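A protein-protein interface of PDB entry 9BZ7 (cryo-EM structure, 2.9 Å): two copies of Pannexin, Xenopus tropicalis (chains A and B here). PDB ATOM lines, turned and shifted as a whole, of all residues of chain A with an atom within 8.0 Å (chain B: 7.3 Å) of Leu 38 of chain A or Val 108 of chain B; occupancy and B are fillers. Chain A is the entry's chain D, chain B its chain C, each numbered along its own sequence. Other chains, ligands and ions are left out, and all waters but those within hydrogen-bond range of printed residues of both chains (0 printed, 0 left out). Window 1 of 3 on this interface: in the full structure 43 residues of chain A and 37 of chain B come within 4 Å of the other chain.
Of chain B, only Val 108 (3.8 Å) comes within 4 Å of Leu 38 of chain A.
Of chain A, only Leu 38 (3.8 Å) comes within 4 Å of Val 108 of chain B.
No residue of chain A comes within 4 Å of Ala 107 of chain B.
Of the printed residues of chain B, Leu 42 of chain A touches Leu 104 (3.5 Å).
Printed residues of chain B within 4 Å of Ile 31 of chain A: Leu 112.
Printed residues of chain A within 4 Å of Leu 112 of chain B: Ile 31 (3.9 Å).
The nearest residue of chain B that does not touch Leu 38 of chain A is Leu 104 of chain B (4.5 Å).
The nearest residue of chain A that does not touch Val 108 of chain B is Leu 35 of chain A (5.4 Å).
Leu 112 of chain B touches Ile 31 of chain A.
Leu 38 of chain A touches Val 108 of chain B (CD1 to CG2, 3.8 Å).
CD2 of Leu 42 of chain A touches CD2 of Leu 104 of chain B (3.5 Å).
Hydrophobic or aromatic side chains of chain A within 4 Å of the printed part of chain B: Ile 31, Leu 38 and Leu 42.
Of the 17 printed residues of chain B, 3 touch a printed residue of chain A.
Printed residues of chain B that touch a printed residue of chain A: Leu 104, Val 108 and Leu 112.
Along chain B the printed residues that touch a printed residue of chain A span positions 104 to 112.
Among the printed residues, no Asp or Glu carboxylate lies within 4 Å of a Lys or Arg side-chain nitrogen of the other chain.
Positions printed for both chains: 33, 36, 37 and 107.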
ATOM      1  N   ILE A  31      -3.813 -11.310  12.587  1.00  0.00           N
ATOM      2  CA  ILE A  31      -3.418 -11.342  11.180  1.00  0.00           C
ATOM      3  C   ILE A  31      -2.629 -10.086  10.822  1.00  0.00           C
ATOM      4  O   ILE A  31      -1.532 -10.159  10.248  1.00  0.00           O
ATOM      5  CB  ILE A  31      -4.655 -11.507  10.278  1.00  0.00           C
ATOM      6  CG1 ILE A  31      -5.210 -12.928  10.393  1.00  0.00           C
ATOM      7  CG2 ILE A  31      -4.309 -11.183   8.833  1.00  0.00           C
ATOM      8  CD1 ILE A  31      -6.406 -13.191   9.501  1.00  0.00           C
ATOM      9  N   VAL A  33      -0.925  -8.144  12.564  1.00  0.00           N
ATOM     10  CA  VAL A  33       0.392  -8.055  13.187  1.00  0.00           C
ATOM     11  C   VAL A  33       1.337  -9.121  12.642  1.00  0.00           C
ATOM     12  O   VAL A  33       2.496  -8.829  12.335  1.00  0.00           O
ATOM     13  CB  VAL A  33       0.256  -8.148  14.720  1.00  0.00           C
ATOM     14  CG1 VAL A  33       1.620  -8.336  15.367  1.00  0.00           C
ATOM     15  CG2 VAL A  33      -0.420  -6.899  15.264  1.00  0.00           C
ATOM     16  N   GLY A  34       0.864 -10.362  12.504  1.00  0.00           N
ATOM     17  CA  GLY A  34       1.740 -11.438  12.077  1.00  0.00           C
ATOM     18  C   GLY A  34       2.189 -11.322  10.634  1.00  0.00           C
ATOM     19  O   GLY A  34       3.353 -11.589  10.320  1.00  0.00           O
ATOM     20  N   LEU A  35       1.280 -10.938   9.732  1.00  0.00           N
ATOM     21  CA  LEU A  35       1.636 -10.908   8.314  1.00  0.00           C
ATOM     22  C   LEU A  35       2.777  -9.943   8.008  1.00  0.00           C
ATOM     23  O   LEU A  35       3.754 -10.365   7.362  1.00  0.00           O
ATOM     24  CB  LEU A  35       0.391 -10.599   7.475  1.00  0.00           C
ATOM     25  CG  LEU A  35       0.612 -10.523   5.962  1.00  0.00           C
ATOM     26  CD1 LEU A  35       0.348 -11.870   5.308  1.00  0.00           C
ATOM     27  CD2 LEU A  35      -0.260  -9.438   5.345  1.00  0.00           C
ATOM     28  N   PRO A  36       2.739  -8.666   8.423  1.00  0.00           N
ATOM     29  CA  PRO A  36       3.896  -7.797   8.150  1.00  0.00           C
ATOM     30  C   PRO A  36       5.181  -8.282   8.795  1.00  0.00           C
ATOM     31  O   PRO A  36       6.245  -8.197   8.172  1.00  0.00           O
ATOM     32  CB  PRO A  36       3.455  -6.437   8.714  1.00  0.00           C
ATOM     33  CG  PRO A  36       1.974  -6.499   8.748  1.00  0.00           C
ATOM     34  CD  PRO A  36       1.653  -7.920   9.083  1.00  0.00           C
ATOM     35  N   LEU A  37       5.114  -8.799  10.023  1.00  0.00           N
ATOM     36  CA  LEU A  37       6.327  -9.262  10.693  1.00  0.00           C
ATOM     37  C   LEU A  37       6.986 -10.389   9.908  1.00  0.00           C
ATOM     38  O   LEU A  37       8.190 -10.346   9.625  1.00  0.00           O
ATOM     39  CB  LEU A  37       5.998  -9.713  12.118  1.00  0.00           C
ATOM     40  CG  LEU A  37       5.842  -8.615  13.173  1.00  0.00           C
ATOM     41  CD1 LEU A  37       5.999  -9.183  14.576  1.00  0.00           C
ATOM     42  CD2 LEU A  37       6.837  -7.490  12.934  1.00  0.00           C
ATOM     43  N   LEU A  38       6.199 -11.396   9.523  1.00  0.00           N
ATOM     44  CA  LEU A  38       6.740 -12.511   8.753  1.00  0.00           C
ATOM     45  C   LEU A  38       7.248 -12.051   7.393  1.00  0.00           C
ATOM     46  O   LEU A  38       8.295 -12.518   6.925  1.00  0.00           O
ATOM     47  CB  LEU A  38       5.678 -13.599   8.590  1.00  0.00           C
ATOM     48  CG  LEU A  38       5.269 -14.346   9.862  1.00  0.00           C
ATOM     49  CD1 LEU A  38       4.233 -15.416   9.554  1.00  0.00           C
ATOM     50  CD2 LEU A  38       6.487 -14.951  10.544  1.00  0.00           C
ATOM     51  N   LEU A  39       6.530 -11.130   6.745  1.00  0.00           N
ATOM     52  CA  LEU A  39       6.937 -10.709   5.408  1.00  0.00           C
ATOM     53  C   LEU A  39       8.243  -9.919   5.437  1.00  0.00           C
ATOM     54  O   LEU A  39       9.102 -10.106   4.567  1.00  0.00           O
ATOM     55  CB  LEU A  39       5.818  -9.908   4.744  1.00  0.00           C
ATOM     56  CG  LEU A  39       5.072 -10.711   3.675  1.00  0.00           C
ATOM     57  CD1 LEU A  39       4.720 -12.101   4.187  1.00  0.00           C
ATOM     58  CD2 LEU A  39       3.823  -9.993   3.205  1.00  0.00           C
ATOM     59  N   ILE A  40       8.432  -9.047   6.431  1.00  0.00           N
ATOM     60  CA  ILE A  40       9.705  -8.329   6.491  1.00  0.00           C
ATOM     61  C   ILE A  40      10.817  -9.222   7.025  1.00  0.00           C
ATOM     62  O   ILE A  40      11.992  -9.003   6.712  1.00  0.00           O
ATOM     63  CB  ILE A  40       9.590  -7.026   7.301  1.00  0.00           C
ATOM     64  CG1 ILE A  40       9.855  -7.272   8.789  1.00  0.00           C
ATOM     65  CG2 ILE A  40       8.272  -6.347   7.040  1.00  0.00           C
ATOM     66  CD1 ILE A  40      10.098  -6.006   9.569  1.00  0.00           C
ATOM     67  N   SER A  41      10.487 -10.248   7.817  1.00  0.00           N
ATOM     68  CA  SER A  41      11.500 -11.244   8.146  1.00  0.00           C
ATOM     69  C   SER A  41      11.982 -11.948   6.884  1.00  0.00           C
ATOM     70  O   SER A  41      13.187 -12.162   6.695  1.00  0.00           O
ATOM     71  CB  SER A  41      10.940 -12.256   9.148  1.00  0.00           C
ATOM     72  OG  SER A  41      10.379 -11.607  10.274  1.00  0.00           O
ATOM     73  N   LEU A  42      11.043 -12.293   6.000  1.00  0.00           N
ATOM     74  CA  LEU A  42      11.393 -12.877   4.710  1.00  0.00           C
ATOM     75  C   LEU A  42      12.224 -11.917   3.870  1.00  0.00           C
ATOM     76  O   LEU A  42      13.182 -12.332   3.215  1.00  0.00           O
ATOM     77  CB  LEU A  42      10.119 -13.281   3.969  1.00  0.00           C
ATOM     78  CG  LEU A  42       9.813 -14.772   3.993  1.00  0.00           C
ATOM     79  CD1 LEU A  42      10.955 -15.529   3.369  1.00  0.00           C
ATOM     80  CD2 LEU A  42       9.631 -15.217   5.429  1.00  0.00           C
ATOM     81  N   ALA A  43      11.863 -10.634   3.868  1.00  0.00           N
ATOM     82  CA  ALA A  43      12.625  -9.649   3.102  1.00  0.00           C
ATOM     83  C   ALA A  43      14.051  -9.513   3.630  1.00  0.00           C
ATOM     84  O   ALA A  43      15.009  -9.439   2.847  1.00  0.00           O
ATOM     85  CB  ALA A  43      11.910  -8.298   3.128  1.00  0.00           C
ATOM     86  N   PHE A  44      14.210  -9.474   4.954  1.00  0.00           N
ATOM     87  CA  PHE A  44      15.541  -9.382   5.544  1.00  0.00           C
ATOM     88  C   PHE A  44      16.372 -10.611   5.213  1.00  0.00           C
ATOM     89  O   PHE A  44      17.540 -10.497   4.817  1.00  0.00           O
ATOM     90  CB  PHE A  44      15.435  -9.201   7.057  1.00  0.00           C
ATOM     91  CG  PHE A  44      15.184  -7.787   7.478  1.00  0.00           C
ATOM     92  CD1 PHE A  44      14.873  -6.819   6.540  1.00  0.00           C
ATOM     93  CD2 PHE A  44      15.270  -7.423   8.811  1.00  0.00           C
ATOM     94  CE1 PHE A  44      14.648  -5.517   6.921  1.00  0.00           C
ATOM     95  CE2 PHE A  44      15.044  -6.120   9.196  1.00  0.00           C
ATOM     96  CZ  PHE A  44      14.733  -5.166   8.250  1.00  0.00           C
ATOM     97  N   ALA A  45      15.779 -11.798   5.356  1.00  0.00           N
ATOM     98  CA  ALA A  45      16.495 -13.020   5.010  1.00  0.00           C
ATOM     99  C   ALA A  45      16.875 -13.034   3.535  1.00  0.00           C
ATOM    100  O   ALA A  45      18.001 -13.398   3.185  1.00  0.00           O
ATOM    101  CB  ALA A  45      15.649 -14.244   5.364  1.00  0.00           C
ATOM    102  N   ALA A 107       3.318  -2.331  11.767  1.00  0.00           N
ATOM    103  CA  ALA A 107       3.046  -3.509  12.585  1.00  0.00           C
ATOM    104  C   ALA A 107       3.040  -3.165  14.070  1.00  0.00           C
ATOM    105  O   ALA A 107       2.163  -3.615  14.818  1.00  0.00           O
ATOM    106  CB  ALA A 107       4.074  -4.601  12.289  1.00  0.00           C
ATOM    107  N   LEU A 268       5.358  -8.522  -1.962  1.00  0.00           N
ATOM    108  CA  LEU A 268       4.996  -8.329  -0.561  1.00  0.00           C
ATOM    109  C   LEU A 268       3.952  -7.230  -0.408  1.00  0.00           C
ATOM    110  O   LEU A 268       3.015  -7.357   0.390  1.00  0.00           O
ATOM    111  CB  LEU A 268       6.240  -8.009   0.268  1.00  0.00           C
ATOM    112  CG  LEU A 268       7.340  -9.072   0.315  1.00  0.00           C
ATOM    113  CD1 LEU A 268       8.301  -8.802   1.464  1.00  0.00           C
ATOM    114  CD2 LEU A 268       6.749 -10.470   0.421  1.00  0.00           C
ATOM    115  N   ASN A 272       0.245  -7.732   1.179  1.00  0.00           N
ATOM    116  CA  ASN A 272      -0.206  -6.906   2.295  1.00  0.00           C
ATOM    117  C   ASN A 272      -1.463  -6.127   1.933  1.00  0.00           C
ATOM    118  O   ASN A 272      -2.394  -6.034   2.739  1.00  0.00           O
ATOM    119  CB  ASN A 272       0.903  -5.948   2.727  1.00  0.00           C
ATOM    120  CG  ASN A 272       1.673  -6.446   3.932  1.00  0.00           C
ATOM    121  OD1 ASN A 272       1.223  -6.311   5.070  1.00  0.00           O
ATOM    122  ND2 ASN A 272       2.853  -6.999   3.692  1.00  0.00           N
ATOM    123  N   ILE A 275      -4.499  -8.530   1.820  1.00  0.00           N
ATOM    124  CA  ILE A 275      -4.906  -8.930   3.165  1.00  0.00           C
ATOM    125  C   ILE A 275      -5.583  -7.771   3.889  1.00  0.00           C
ATOM    126  O   ILE A 275      -6.602  -7.953   4.567  1.00  0.00           O
ATOM    127  CB  ILE A 275      -3.694  -9.463   3.953  1.00  0.00           C
ATOM    128  CG1 ILE A 275      -3.198 -10.775   3.342  1.00  0.00           C
ATOM    129  CG2 ILE A 275      -4.047  -9.657   5.420  1.00  0.00           C
ATOM    130  CD1 ILE A 275      -4.180 -11.918   3.469  1.00  0.00           C
ATOM    131  N   ALA B  32       0.306 -30.518   6.512  1.00  0.00           N
ATOM    132  CA  ALA B  32       0.277 -29.461   5.510  1.00  0.00           C
ATOM    133  C   ALA B  32       0.933 -28.176   5.992  1.00  0.00           C
ATOM    134  O   ALA B  32       1.262 -27.317   5.167  1.00  0.00           O
ATOM    135  CB  ALA B  32      -1.166 -29.179   5.086  1.00  0.00           C
ATOM    136  N   VAL B  33       1.115 -28.011   7.300  1.00  0.00           N
ATOM    137  CA  VAL B  33       1.850 -26.856   7.805  1.00  0.00           C
ATOM    138  C   VAL B  33       3.331 -27.171   7.979  1.00  0.00           C
ATOM    139  O   VAL B  33       4.189 -26.372   7.595  1.00  0.00           O
ATOM    140  CB  VAL B  33       1.216 -26.363   9.122  1.00  0.00           C
ATOM    141  CG1 VAL B  33       2.120 -25.348   9.803  1.00  0.00           C
ATOM    142  CG2 VAL B  33      -0.154 -25.757   8.853  1.00  0.00           C
ATOM    143  N   PRO B  36       5.763 -27.740   4.272  1.00  0.00           N
ATOM    144  CA  PRO B  36       6.309 -26.552   3.593  1.00  0.00           C
ATOM    145  C   PRO B  36       7.307 -25.781   4.437  1.00  0.00           C
ATOM    146  O   PRO B  36       8.317 -25.307   3.906  1.00  0.00           O
ATOM    147  CB  PRO B  36       5.057 -25.717   3.286  1.00  0.00           C
ATOM    148  CG  PRO B  36       3.935 -26.687   3.305  1.00  0.00           C
ATOM    149  CD  PRO B  36       4.294 -27.673   4.369  1.00  0.00           C
ATOM    150  N   LEU B  37       7.060 -25.648   5.742  1.00  0.00           N
ATOM    151  CA  LEU B  37       7.980 -24.896   6.591  1.00  0.00           C
ATOM    152  C   LEU B  37       9.363 -25.535   6.593  1.00  0.00           C
ATOM    153  O   LEU B  37      10.376 -24.858   6.370  1.00  0.00           O
ATOM    154  CB  LEU B  37       7.423 -24.805   8.013  1.00  0.00           C
ATOM    155  CG  LEU B  37       6.341 -23.752   8.267  1.00  0.00           C
ATOM    156  CD1 LEU B  37       6.225 -23.437   9.752  1.00  0.00           C
ATOM    157  CD2 LEU B  37       6.619 -22.488   7.470  1.00  0.00           C
ATOM    158  N   ILE B 102       6.055 -17.889  -1.833  1.00  0.00           N
ATOM    159  CA  ILE B 102       4.755 -18.506  -2.089  1.00  0.00           C
ATOM    160  C   ILE B 102       4.521 -19.671  -1.137  1.00  0.00           C
ATOM    161  O   ILE B 102       3.407 -19.864  -0.632  1.00  0.00           O
ATOM    162  CB  ILE B 102       4.649 -18.940  -3.563  1.00  0.00           C
ATOM    163  CG1 ILE B 102       4.472 -17.719  -4.472  1.00  0.00           C
ATOM    164  CG2 ILE B 102       3.508 -19.928  -3.759  1.00  0.00           C
ATOM    165  CD1 ILE B 102       3.427 -16.738  -3.980  1.00  0.00           C
ATOM    166  N   LEU B 103       5.558 -20.473  -0.882  1.00  0.00           N
ATOM    167  CA  LEU B 103       5.393 -21.586   0.048  1.00  0.00           C
ATOM    168  C   LEU B 103       5.106 -21.099   1.466  1.00  0.00           C
ATOM    169  O   LEU B 103       4.265 -21.676   2.164  1.00  0.00           O
ATOM    170  CB  LEU B 103       6.620 -22.492   0.017  1.00  0.00           C
ATOM    171  CG  LEU B 103       6.554 -23.726  -0.892  1.00  0.00           C
ATOM    172  CD1 LEU B 103       5.868 -23.431  -2.216  1.00  0.00           C
ATOM    173  CD2 LEU B 103       7.936 -24.307  -1.119  1.00  0.00           C
ATOM    174  N   LEU B 104       5.788 -20.042   1.911  1.00  0.00           N
ATOM    175  CA  LEU B 104       5.449 -19.461   3.210  1.00  0.00           C
ATOM    176  C   LEU B 104       4.021 -18.937   3.233  1.00  0.00           C
ATOM    177  O   LEU B 104       3.310 -19.100   4.232  1.00  0.00           O
ATOM    178  CB  LEU B 104       6.412 -18.338   3.581  1.00  0.00           C
ATOM    179  CG  LEU B 104       6.379 -18.076   5.092  1.00  0.00           C
ATOM    180  CD1 LEU B 104       7.427 -18.863   5.868  1.00  0.00           C
ATOM    181  CD2 LEU B 104       6.459 -16.588   5.387  1.00  0.00           C
ATOM    182  N   LEU B 105       3.592 -18.281   2.153  1.00  0.00           N
ATOM    183  CA  LEU B 105       2.231 -17.759   2.104  1.00  0.00           C
ATOM    184  C   LEU B 105       1.208 -18.882   2.218  1.00  0.00           C
ATOM    185  O   LEU B 105       0.246 -18.777   2.988  1.00  0.00           O
ATOM    186  CB  LEU B 105       2.019 -16.965   0.814  1.00  0.00           C
ATOM    187  CG  LEU B 105       0.585 -16.547   0.487  1.00  0.00           C
ATOM    188  CD1 LEU B 105       0.247 -15.208   1.117  1.00  0.00           C
ATOM    189  CD2 LEU B 105       0.381 -16.497  -1.018  1.00  0.00           C
ATOM    190  N   VAL B 106       1.411 -19.976   1.481  1.00  0.00           N
ATOM    191  CA  VAL B 106       0.448 -21.072   1.539  1.00  0.00           C
ATOM    192  C   VAL B 106       0.505 -21.772   2.895  1.00  0.00           C
ATOM    193  O   VAL B 106      -0.528 -22.214   3.410  1.00  0.00           O
ATOM    194  CB  VAL B 106       0.648 -22.059   0.368  1.00  0.00           C
ATOM    195  CG1 VAL B 106       0.593 -21.326  -0.963  1.00  0.00           C
ATOM    196  CG2 VAL B 106       1.942 -22.842   0.504  1.00  0.00           C
ATOM    197  N   ALA B 107       1.690 -21.869   3.509  1.00  0.00           N
ATOM    198  CA  ALA B 107       1.778 -22.466   4.839  1.00  0.00           C
ATOM    199  C   ALA B 107       1.037 -21.628   5.874  1.00  0.00           C
ATOM    200  O   ALA B 107       0.313 -22.166   6.721  1.00  0.00           O
ATOM    201  CB  ALA B 107       3.244 -22.643   5.236  1.00  0.00           C
ATOM    202  N   VAL B 108       1.205 -20.305   5.823  1.00  0.00           N
ATOM    203  CA  VAL B 108       0.506 -19.428   6.756  1.00  0.00           C
ATOM    204  C   VAL B 108      -0.999 -19.486   6.519  1.00  0.00           C
ATOM    205  O   VAL B 108      -1.794 -19.521   7.468  1.00  0.00           O
ATOM    206  CB  VAL B 108       1.050 -17.992   6.642  1.00  0.00           C
ATOM    207  CG1 VAL B 108       0.030 -16.982   7.151  1.00  0.00           C
ATOM    208  CG2 VAL B 108       2.362 -17.862   7.402  1.00  0.00           C
ATOM    209  N   LEU B 109      -1.414 -19.503   5.250  1.00  0.00           N
ATOM    210  CA  LEU B 109      -2.834 -19.605   4.938  1.00  0.00           C
ATOM    211  C   LEU B 109      -3.418 -20.934   5.398  1.00  0.00           C
ATOM    212  O   LEU B 109      -4.594 -20.997   5.768  1.00  0.00           O
ATOM    213  CB  LEU B 109      -3.055 -19.412   3.438  1.00  0.00           C
ATOM    214  CG  LEU B 109      -2.904 -17.984   2.906  1.00  0.00           C
ATOM    215  CD1 LEU B 109      -3.455 -17.876   1.493  1.00  0.00           C
ATOM    216  CD2 LEU B 109      -3.586 -16.987   3.832  1.00  0.00           C
ATOM    217  N   LEU B 110      -2.622 -22.006   5.374  1.00  0.00           N
ATOM    218  CA  LEU B 110      -3.091 -23.294   5.875  1.00  0.00           C
ATOM    219  C   LEU B 110      -3.143 -23.322   7.397  1.00  0.00           C
ATOM    220  O   LEU B 110      -3.983 -24.020   7.974  1.00  0.00           O
ATOM    221  CB  LEU B 110      -2.194 -24.418   5.357  1.00  0.00           C
ATOM    222  CG  LEU B 110      -2.500 -24.936   3.952  1.00  0.00           C
ATOM    223  CD1 LEU B 110      -1.379 -25.834   3.457  1.00  0.00           C
ATOM    224  CD2 LEU B 110      -3.829 -25.671   3.930  1.00  0.00           C
ATOM    225  N   TYR B 111      -2.244 -22.592   8.061  1.00  0.00           N
ATOM    226  CA  TYR B 111      -2.288 -22.504   9.516  1.00  0.00           C
ATOM    227  C   TYR B 111      -3.424 -21.611  10.005  1.00  0.00           C
ATOM    228  O   TYR B 111      -3.884 -21.781  11.139  1.00  0.00           O
ATOM    229  CB  TYR B 111      -0.951 -21.991  10.055  1.00  0.00           C
ATOM    230  CG  TYR B 111      -0.909 -21.845  11.559  1.00  0.00           C
ATOM    231  CD1 TYR B 111      -0.811 -22.959  12.384  1.00  0.00           C
ATOM    232  CD2 TYR B 111      -0.968 -20.592  12.157  1.00  0.00           C
ATOM    233  CE1 TYR B 111      -0.772 -22.830  13.759  1.00  0.00           C
ATOM    234  CE2 TYR B 111      -0.929 -20.453  13.531  1.00  0.00           C
ATOM    235  CZ  TYR B 111      -0.831 -21.574  14.328  1.00  0.00           C
ATOM    236  OH  TYR B 111      -0.794 -21.440  15.697  1.00  0.00           O
ATOM    237  N   LEU B 112      -3.873 -20.666   9.177  1.00  0.00           N
ATOM    238  CA  LEU B 112      -4.929 -19.742   9.593  1.00  0.00           C
ATOM    239  C   LEU B 112      -6.220 -20.432  10.031  1.00  0.00           C
ATOM    240  O   LEU B 112      -6.794 -20.014  11.055  1.00  0.00           O
ATOM    241  CB  LEU B 112      -5.194 -18.737   8.467  1.00  0.00           C
ATOM    242  CG  LEU B 112      -4.354 -17.458   8.460  1.00  0.00           C
ATOM    243  CD1 LEU B 112      -5.079 -16.345   7.721  1.00  0.00           C
ATOM    244  CD2 LEU B 112      -4.003 -17.025   9.877  1.00  0.00           C
ATOM    245  N   PRO B 113      -6.749 -21.442   9.325  1.00  0.00           N
ATOM    246  CA  PRO B 113      -7.993 -22.076   9.796  1.00  0.00           C
ATOM    247  C   PRO B 113      -7.888 -22.682  11.182  1.00  0.00           C
ATOM    248  O   PRO B 113      -8.893 -22.724  11.901  1.00  0.00           O
ATOM    249  CB  PRO B 113      -8.266 -23.147   8.732  1.00  0.00           C
ATOM    250  CG  PRO B 113      -7.598 -22.641   7.519  1.00  0.00           C
ATOM    251  CD  PRO B 113      -6.352 -21.978   8.011  1.00  0.00           C
ATOM    252  N   ILE B 215      -6.932 -23.798  -0.434  1.00  0.00           N
ATOM    253  CA  ILE B 215      -5.513 -23.459  -0.385  1.00  0.00           C
ATOM    254  C   ILE B 215      -4.667 -24.620  -0.893  1.00  0.00           C
ATOM    255  O   ILE B 215      -3.705 -24.424  -1.646  1.00  0.00           O
ATOM    256  CB  ILE B 215      -5.113 -23.040   1.041  1.00  0.00           C
ATOM    257  CG1 ILE B 215      -5.833 -21.751   1.426  1.00  0.00           C
ATOM    258  CG2 ILE B 215      -3.608 -22.849   1.139  1.00  0.00           C
ATOM    259  CD1 ILE B 215      -5.861 -21.502   2.904  1.00  0.00           C
